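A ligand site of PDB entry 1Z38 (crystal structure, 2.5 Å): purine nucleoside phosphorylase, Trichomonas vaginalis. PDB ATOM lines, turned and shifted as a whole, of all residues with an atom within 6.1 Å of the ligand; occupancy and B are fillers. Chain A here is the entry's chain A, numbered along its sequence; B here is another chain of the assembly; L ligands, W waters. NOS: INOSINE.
The side-chain carboxylate of Glu 181 lies within hydrogen-bond range of an oxygen (O2') of the ligand (2.7 Å). A ring nitrogen (NE2) of His 4 of chain B is in hydrogen-bond range of an oxygen (O5') of the ligand, 2.7 Å away. The guanidinium group (NH2) of Arg 43 of chain B lies within hydrogen-bond range of an oxygen (O4') of the ligand, at 3.2 Å. N of Met 180 is in hydrogen-bond range of O2' of the ligand (3.3 Å). The backbone NH (N) of Gly 92 sits at hydrogen-bond distance from a nitrogen (N7) of the ligand, at 3.4 Å.
The backbone NH (N) of Glu 181 is in hydrogen-bond range of the side-chain carboxylate (OE2) of Glu 179 (3.0 Å). The side-chain carboxylate of Glu 181 sits at hydrogen-bond distance from the backbone NH of Gly 65 (3.0 Å). The backbone NH of Gly 65 lies close to the backbone carbonyl oxygen of Met 180 (3.3 Å). The backbone carbonyl oxygen of Cys 91 sits at hydrogen-bond distance from the backbone NH of Ser 203, at 3.0 Å. The backbone carbonyl oxygen (O) of Gly 92 sits at hydrogen-bond distance from the backbone NH (N) of Val 178, 2.7 Å away. The side-chain carboxylate of Glu 179 is in salt-bridge range of the guanidinium group of Arg 87. The backbone NH (N) of Thr 156 is in hydrogen-bond range of the backbone carbonyl oxygen (O) of Glu 179, 3.0 Å away. A ring nitrogen (NE2) of His 62 is in hydrogen-bond range of the guanidinium group (NH1) of Arg 87 (3.0 Å).
Met 64 touches the ligand (CG to O3', 3.5 Å). Arg 87 touches the ligand (NH2 to O2', 3.6 Å). Thr 90 touches the ligand (OG1 to C8, 3.3 Å). Cys 91 touches the ligand. Phe 159 touches the ligand. Val 178 touches the ligand (O to C5, 3.6 Å). Glu 179 touches the ligand (CB to O2', 3.5 Å). Within 4 Å of the ligand: Met 64, Arg 87, Thr 90, Cys 91, Gly 92, Phe 159, Val 178, Glu 179, Met 180, Glu 181, His 4 of chain B and Arg 43 of chain B.
Water W4 bridges an oxygen (O3') of the ligand (2.7 Å) and the guanidinium group (NH1) of Arg 43 of chain B (2.9 Å). Water W3 bridges O5' of the ligand (2.9 Å) and NH2 of Arg 43 of chain B (3.4 Å). Water W1 lies within hydrogen-bond range of the backbone carbonyl oxygen (O) of Phe 159 (2.8 Å) and a nitrogen (N1) of the ligand (3.2 Å). Water W2 lies within hydrogen-bond range of the side-chain hydroxyl of Thr 90 (2.8 Å) and an oxygen (O4') of the ligand (3.5 Å).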
ATOM      1  N   GLY A  20      22.835  18.737 -28.933  1.00  0.00           N
ATOM      2  CA  GLY A  20      23.515  19.332 -27.793  1.00  0.00           C
ATOM      3  C   GLY A  20      23.030  18.815 -26.459  1.00  0.00           C
ATOM      4  O   GLY A  20      23.835  18.455 -25.596  1.00  0.00           O
ATOM      5  N   HIS A  62      26.449  16.290 -27.712  1.00  0.00           N
ATOM      6  CA  HIS A  62      27.735  16.840 -28.133  1.00  0.00           C
ATOM      7  C   HIS A  62      28.018  18.186 -27.466  1.00  0.00           C
ATOM      8  O   HIS A  62      28.948  18.887 -27.844  1.00  0.00           O
ATOM      9  CB  HIS A  62      27.799  16.995 -29.655  1.00  0.00           C
ATOM     10  CG  HIS A  62      26.736  17.871 -30.232  1.00  0.00           C
ATOM     11  ND1 HIS A  62      26.484  19.151 -29.771  1.00  0.00           N
ATOM     12  CD2 HIS A  62      25.874  17.673 -31.257  1.00  0.00           C
ATOM     13  CE1 HIS A  62      25.513  19.700 -30.492  1.00  0.00           C
ATOM     14  NE2 HIS A  62      25.127  18.817 -31.394  1.00  0.00           N
ATOM     15  N   GLY A  63      27.212  18.528 -26.468  1.00  0.00           N
ATOM     16  CA  GLY A  63      27.393  19.793 -25.762  1.00  0.00           C
ATOM     17  C   GLY A  63      27.110  20.996 -26.648  1.00  0.00           C
ATOM     18  O   GLY A  63      26.706  20.847 -27.793  1.00  0.00           O
ATOM     19  N   MET A  64      27.335  22.194 -26.121  1.00  0.00           N
ATOM     20  CA  MET A  64      27.092  23.413 -26.896  1.00  0.00           C
ATOM     21  C   MET A  64      28.409  24.064 -27.311  1.00  0.00           C
ATOM     22  O   MET A  64      29.340  24.151 -26.505  1.00  0.00           O
ATOM     23  CB  MET A  64      26.271  24.414 -26.088  1.00  0.00           C
ATOM     24  CG  MET A  64      24.921  23.905 -25.614  1.00  0.00           C
ATOM     25  SD  MET A  64      23.995  25.168 -24.712  1.00  0.00           S
ATOM     26  CE  MET A  64      24.934  25.248 -23.159  1.00  0.00           C
ATOM     27  N   GLY A  65      28.498  24.503 -28.562  1.00  0.00           N
ATOM     28  CA  GLY A  65      29.701  25.171 -29.040  1.00  0.00           C
ATOM     29  C   GLY A  65      30.616  24.330 -29.905  1.00  0.00           C
ATOM     30  O   GLY A  65      30.694  23.108 -29.743  1.00  0.00           O
ATOM     31  N   ARG A  87      23.765  16.000 -37.396  1.00  0.00           N
ATOM     32  CA  ARG A  87      23.436  16.848 -36.255  1.00  0.00           C
ATOM     33  C   ARG A  87      21.945  17.173 -36.299  1.00  0.00           C
ATOM     34  O   ARG A  87      21.403  17.623 -37.306  1.00  0.00           O
ATOM     35  CB  ARG A  87      24.252  18.149 -36.292  1.00  0.00           C
ATOM     36  CG  ARG A  87      24.500  18.736 -34.905  1.00  0.00           C
ATOM     37  CD  ARG A  87      25.176  20.090 -34.986  1.00  0.00           C
ATOM     38  NE  ARG A  87      24.196  21.181 -35.010  1.00  0.00           N
ATOM     39  CZ  ARG A  87      23.374  21.454 -34.005  1.00  0.00           C
ATOM     40  NH1 ARG A  87      23.410  20.730 -32.894  1.00  0.00           N
ATOM     41  NH2 ARG A  87      22.506  22.457 -34.103  1.00  0.00           N
ATOM     42  N   THR A  90      18.101  22.359 -32.403  1.00  0.00           N
ATOM     43  CA  THR A  90      17.286  23.566 -32.480  1.00  0.00           C
ATOM     44  C   THR A  90      18.186  24.700 -32.967  1.00  0.00           C
ATOM     45  O   THR A  90      19.407  24.576 -32.947  1.00  0.00           O
ATOM     46  CB  THR A  90      16.717  23.925 -31.105  1.00  0.00           C
ATOM     47  OG1 THR A  90      17.789  24.231 -30.202  1.00  0.00           O
ATOM     48  CG2 THR A  90      15.905  22.754 -30.551  1.00  0.00           C
ATOM     49  N   CYS A  91      17.577  25.796 -33.401  1.00  0.00           N
ATOM     50  CA  CYS A  91      18.342  26.939 -33.879  1.00  0.00           C
ATOM     51  C   CYS A  91      17.509  28.213 -33.815  1.00  0.00           C
ATOM     52  O   CYS A  91      16.289  28.159 -33.620  1.00  0.00           O
ATOM     53  CB  CYS A  91      18.808  26.687 -35.330  1.00  0.00           C
ATOM     54  SG  CYS A  91      17.469  26.404 -36.540  1.00  0.00           S
ATOM     55  N   GLY A  92      18.168  29.359 -33.965  1.00  0.00           N
ATOM     56  CA  GLY A  92      17.475  30.641 -33.926  1.00  0.00           C
ATOM     57  C   GLY A  92      17.371  31.231 -35.326  1.00  0.00           C
ATOM     58  O   GLY A  92      18.376  31.458 -35.987  1.00  0.00           O
ATOM     59  N   ALA A  93      16.136  31.479 -35.768  1.00  0.00           N
ATOM     60  CA  ALA A  93      15.915  32.028 -37.097  1.00  0.00           C
ATOM     61  C   ALA A  93      16.556  33.402 -37.265  1.00  0.00           C
ATOM     62  O   ALA A  93      16.559  34.214 -36.339  1.00  0.00           O
ATOM     63  CB  ALA A  93      14.421  32.122 -37.390  1.00  0.00           C
ATOM     64  N   THR A 156      27.605  30.316 -34.130  1.00  0.00           N
ATOM     65  CA  THR A 156      28.192  31.368 -33.326  1.00  0.00           C
ATOM     66  C   THR A 156      28.922  30.833 -32.096  1.00  0.00           C
ATOM     67  O   THR A 156      28.601  29.755 -31.580  1.00  0.00           O
ATOM     68  CB  THR A 156      27.114  32.373 -32.849  1.00  0.00           C
ATOM     69  OG1 THR A 156      27.743  33.478 -32.198  1.00  0.00           O
ATOM     70  CG2 THR A 156      26.147  31.700 -31.866  1.00  0.00           C
ATOM     71  N   LEU A 158      29.166  32.976 -29.671  1.00  0.00           N
ATOM     72  CA  LEU A 158      28.483  33.813 -28.678  1.00  0.00           C
ATOM     73  C   LEU A 158      26.960  33.765 -28.766  1.00  0.00           C
ATOM     74  O   LEU A 158      26.356  34.480 -29.571  1.00  0.00           O
ATOM     75  CB  LEU A 158      28.941  35.273 -28.842  1.00  0.00           C
ATOM     76  CG  LEU A 158      30.122  35.875 -28.064  1.00  0.00           C
ATOM     77  CD1 LEU A 158      30.848  34.816 -27.266  1.00  0.00           C
ATOM     78  CD2 LEU A 158      31.066  36.577 -29.022  1.00  0.00           C
ATOM     79  N   PHE A 159      26.339  32.926 -27.933  1.00  0.00           N
ATOM     80  CA  PHE A 159      24.889  32.849 -27.895  1.00  0.00           C
ATOM     81  C   PHE A 159      24.402  34.284 -27.670  1.00  0.00           C
ATOM     82  O   PHE A 159      23.499  34.773 -28.359  1.00  0.00           O
ATOM     83  CB  PHE A 159      24.429  31.959 -26.748  1.00  0.00           C
ATOM     84  CG  PHE A 159      22.930  31.797 -26.665  1.00  0.00           C
ATOM     85  CD1 PHE A 159      22.283  30.793 -27.381  1.00  0.00           C
ATOM     86  CD2 PHE A 159      22.164  32.666 -25.882  1.00  0.00           C
ATOM     87  CE1 PHE A 159      20.899  30.656 -27.326  1.00  0.00           C
ATOM     88  CE2 PHE A 159      20.792  32.531 -25.814  1.00  0.00           C
ATOM     89  CZ  PHE A 159      20.144  31.526 -26.530  1.00  0.00           C
ATOM     90  N   VAL A 178      20.714  30.318 -36.742  1.00  0.00           N
ATOM     91  CA  VAL A 178      21.938  30.264 -35.964  1.00  0.00           C
ATOM     92  C   VAL A 178      21.936  29.113 -34.969  1.00  0.00           C
ATOM     93  O   VAL A 178      20.935  28.872 -34.295  1.00  0.00           O
ATOM     94  CB  VAL A 178      22.158  31.559 -35.133  1.00  0.00           C
ATOM     95  CG1 VAL A 178      23.460  31.446 -34.325  1.00  0.00           C
ATOM     96  CG2 VAL A 178      22.202  32.763 -36.038  1.00  0.00           C
ATOM     97  N   GLU A 179      23.064  28.425 -34.893  1.00  0.00           N
ATOM     98  CA  GLU A 179      23.239  27.347 -33.926  1.00  0.00           C
ATOM     99  C   GLU A 179      24.697  27.474 -33.456  1.00  0.00           C
ATOM    100  O   GLU A 179      25.279  28.559 -33.585  1.00  0.00           O
ATOM    101  CB  GLU A 179      22.900  25.964 -34.523  1.00  0.00           C
ATOM    102  CG  GLU A 179      23.386  25.690 -35.927  1.00  0.00           C
ATOM    103  CD  GLU A 179      24.863  25.383 -35.982  1.00  0.00           C
ATOM    104  OE1 GLU A 179      25.655  26.323 -36.234  1.00  0.00           O
ATOM    105  OE2 GLU A 179      25.246  24.205 -35.771  1.00  0.00           O
ATOM    106  N   MET A 180      25.289  26.412 -32.933  1.00  0.00           N
ATOM    107  CA  MET A 180      26.657  26.555 -32.416  1.00  0.00           C
ATOM    108  C   MET A 180      27.581  25.351 -32.631  1.00  0.00           C
ATOM    109  O   MET A 180      28.483  25.130 -31.833  1.00  0.00           O
ATOM    110  CB  MET A 180      26.595  26.871 -30.914  1.00  0.00           C
ATOM    111  CG  MET A 180      25.788  28.133 -30.569  1.00  0.00           C
ATOM    112  SD  MET A 180      25.567  28.481 -28.796  1.00  0.00           S
ATOM    113  CE  MET A 180      27.231  28.878 -28.286  1.00  0.00           C
ATOM    114  N   GLU A 181      27.384  24.596 -33.703  1.00  0.00           N
ATOM    115  CA  GLU A 181      28.212  23.423 -33.898  1.00  0.00           C
ATOM    116  C   GLU A 181      28.609  23.068 -35.329  1.00  0.00           C
ATOM    117  O   GLU A 181      29.742  22.668 -35.579  1.00  0.00           O
ATOM    118  CB  GLU A 181      27.523  22.206 -33.254  1.00  0.00           C
ATOM    119  CG  GLU A 181      27.363  22.313 -31.732  1.00  0.00           C
ATOM    120  CD  GLU A 181      26.196  23.180 -31.298  1.00  0.00           C
ATOM    121  OE1 GLU A 181      26.130  23.536 -30.101  1.00  0.00           O
ATOM    122  OE2 GLU A 181      25.337  23.514 -32.141  1.00  0.00           O
ATOM    123  N   SER A 203      13.488  27.238 -32.928  1.00  0.00           N
ATOM    124  CA  SER A 203      12.812  27.365 -31.648  1.00  0.00           C
ATOM    125  C   SER A 203      12.384  28.807 -31.344  1.00  0.00           C
ATOM    126  O   SER A 203      11.591  29.040 -30.423  1.00  0.00           O
ATOM    127  CB  SER A 203      13.715  26.828 -30.525  1.00  0.00           C
ATOM    128  OG  SER A 203      14.992  27.428 -30.587  1.00  0.00           O
ATOM    129  N   ASP A 204      12.907  29.760 -32.111  1.00  0.00           N
ATOM    130  CA  ASP A 204      12.564  31.162 -31.941  1.00  0.00           C
ATOM    131  C   ASP A 204      13.238  32.004 -33.016  1.00  0.00           C
ATOM    132  O   ASP A 204      14.095  31.519 -33.747  1.00  0.00           O
ATOM    133  CB  ASP A 204      12.987  31.654 -30.551  1.00  0.00           C
ATOM    134  CG  ASP A 204      12.243  32.909 -30.114  1.00  0.00           C
ATOM    135  OD1 ASP A 204      11.348  33.381 -30.855  1.00  0.00           O
ATOM    136  OD2 ASP A 204      12.536  33.421 -29.006  1.00  0.00           O
ATOM    137  N   ILE A 206      15.444  35.498 -33.786  1.00  0.00           N
ATOM    138  CA  ILE A 206      16.288  36.473 -33.110  1.00  0.00           C
ATOM    139  C   ILE A 206      15.987  37.928 -33.442  1.00  0.00           C
ATOM    140  O   ILE A 206      16.353  38.829 -32.680  1.00  0.00           O
ATOM    141  CB  ILE A 206      17.803  36.207 -33.374  1.00  0.00           C
ATOM    142  CG1 ILE A 206      18.142  36.514 -34.826  1.00  0.00           C
ATOM    143  CG2 ILE A 206      18.133  34.758 -33.046  1.00  0.00           C
ATOM    144  CD1 ILE A 206      19.615  36.310 -35.161  1.00  0.00           C
ATOM    145  N   PRO B   3      16.971  30.261 -21.353  1.00  0.00           N
ATOM    146  CA  PRO B   3      16.918  29.105 -22.257  1.00  0.00           C
ATOM    147  C   PRO B   3      17.722  27.907 -21.744  1.00  0.00           C
ATOM    148  O   PRO B   3      17.545  26.795 -22.238  1.00  0.00           O
ATOM    149  CB  PRO B   3      17.502  29.662 -23.552  1.00  0.00           C
ATOM    150  CG  PRO B   3      17.125  31.114 -23.497  1.00  0.00           C
ATOM    151  CD  PRO B   3      17.428  31.465 -22.068  1.00  0.00           C
ATOM    152  N   HIS B   4      18.603  28.133 -20.770  1.00  0.00           N
ATOM    153  CA  HIS B   4      19.436  27.041 -20.257  1.00  0.00           C
ATOM    154  C   HIS B   4      19.339  26.837 -18.747  1.00  0.00           C
ATOM    155  O   HIS B   4      20.052  26.007 -18.181  1.00  0.00           O
ATOM    156  CB  HIS B   4      20.896  27.277 -20.625  1.00  0.00           C
ATOM    157  CG  HIS B   4      21.093  27.811 -22.008  1.00  0.00           C
ATOM    158  ND1 HIS B   4      21.015  29.157 -22.308  1.00  0.00           N
ATOM    159  CD2 HIS B   4      21.344  27.173 -23.181  1.00  0.00           C
ATOM    160  CE1 HIS B   4      21.197  29.322 -23.602  1.00  0.00           C
ATOM    161  NE2 HIS B   4      21.388  28.137 -24.152  1.00  0.00           N
ATOM    162  N   ARG B  43      19.197  20.433 -19.893  1.00  0.00           N
ATOM    163  CA  ARG B  43      20.327  19.829 -20.606  1.00  0.00           C
ATOM    164  C   ARG B  43      21.206  19.009 -19.661  1.00  0.00           C
ATOM    165  O   ARG B  43      22.389  18.814 -19.917  1.00  0.00           O
ATOM    166  CB  ARG B  43      21.171  20.920 -21.288  1.00  0.00           C
ATOM    167  CG  ARG B  43      20.447  21.631 -22.420  1.00  0.00           C
ATOM    168  CD  ARG B  43      21.203  22.866 -22.900  1.00  0.00           C
ATOM    169  NE  ARG B  43      20.537  23.487 -24.042  1.00  0.00           N
ATOM    170  CZ  ARG B  43      20.710  23.114 -25.311  1.00  0.00           C
ATOM    171  NH1 ARG B  43      21.555  22.139 -25.615  1.00  0.00           N
ATOM    172  NH2 ARG B  43      20.039  23.716 -26.275  1.00  0.00           N
ATOM    173  N   ILE B  71      27.864  30.967 -21.989  1.00  0.00           N
ATOM    174  CA  ILE B  71      26.417  31.017 -21.876  1.00  0.00           C
ATOM    175  C   ILE B  71      25.997  30.967 -20.391  1.00  0.00           C
ATOM    176  O   ILE B  71      25.232  31.810 -19.909  1.00  0.00           O
ATOM    177  CB  ILE B  71      25.760  29.840 -22.626  1.00  0.00           C
ATOM    178  CG1 ILE B  71      25.837  30.090 -24.138  1.00  0.00           C
ATOM    179  CG2 ILE B  71      24.334  29.642 -22.167  1.00  0.00           C
ATOM    180  CD1 ILE B  71      25.518  28.870 -24.975  1.00  0.00           C
HETATM  181  N9  NOS L   1      20.539  27.000 -30.431  1.00  0.00           N
HETATM  182  C4  NOS L   1      21.103  28.192 -30.603  1.00  0.00           C
HETATM  183  N3  NOS L   1      22.388  28.594 -30.595  1.00  0.00           N
HETATM  184  C2  NOS L   1      22.721  29.857 -30.778  1.00  0.00           C
HETATM  185  N1  NOS L   1      21.744  30.823 -30.999  1.00  0.00           N
HETATM  186  C6  NOS L   1      20.391  30.444 -31.020  1.00  0.00           C
HETATM  187  O6  NOS L   1      19.507  31.275 -31.208  1.00  0.00           O
HETATM  188  C5  NOS L   1      20.076  29.105 -30.820  1.00  0.00           C
HETATM  189  N7  NOS L   1      18.937  28.425 -30.772  1.00  0.00           N
HETATM  190  C8  NOS L   1      19.221  27.146 -30.531  1.00  0.00           C
HETATM  191  C5' NOS L   1      22.065  27.345 -27.716  1.00  0.00           C
HETATM  192  O5' NOS L   1      20.992  27.449 -26.779  1.00  0.00           O
HETATM  193  C4' NOS L   1      22.229  25.878 -28.123  1.00  0.00           C
HETATM  194  O4' NOS L   1      21.081  25.327 -28.796  1.00  0.00           O
HETATM  195  C1' NOS L   1      21.209  25.703 -30.176  1.00  0.00           C
HETATM  196  C2' NOS L   1      22.720  25.741 -30.457  1.00  0.00           C
HETATM  197  O2' NOS L   1      23.092  24.622 -31.271  1.00  0.00           O
HETATM  198  C3' NOS L   1      23.383  25.611 -29.084  1.00  0.00           C
HETATM  199  O3' NOS L   1      23.875  24.290 -28.899  1.00  0.00           O
HETATM  200  O   HOH W   1      22.781  33.800 -30.912  1.00  0.00           O
HETATM  201  O   HOH W   2      19.736  22.228 -29.697  1.00  0.00           O
HETATM  202  O   HOH W   3      18.203  26.547 -26.736  1.00  0.00           O
HETATM  203  O   HOH W   4      22.349  22.169 -28.403  1.00  0.00           O
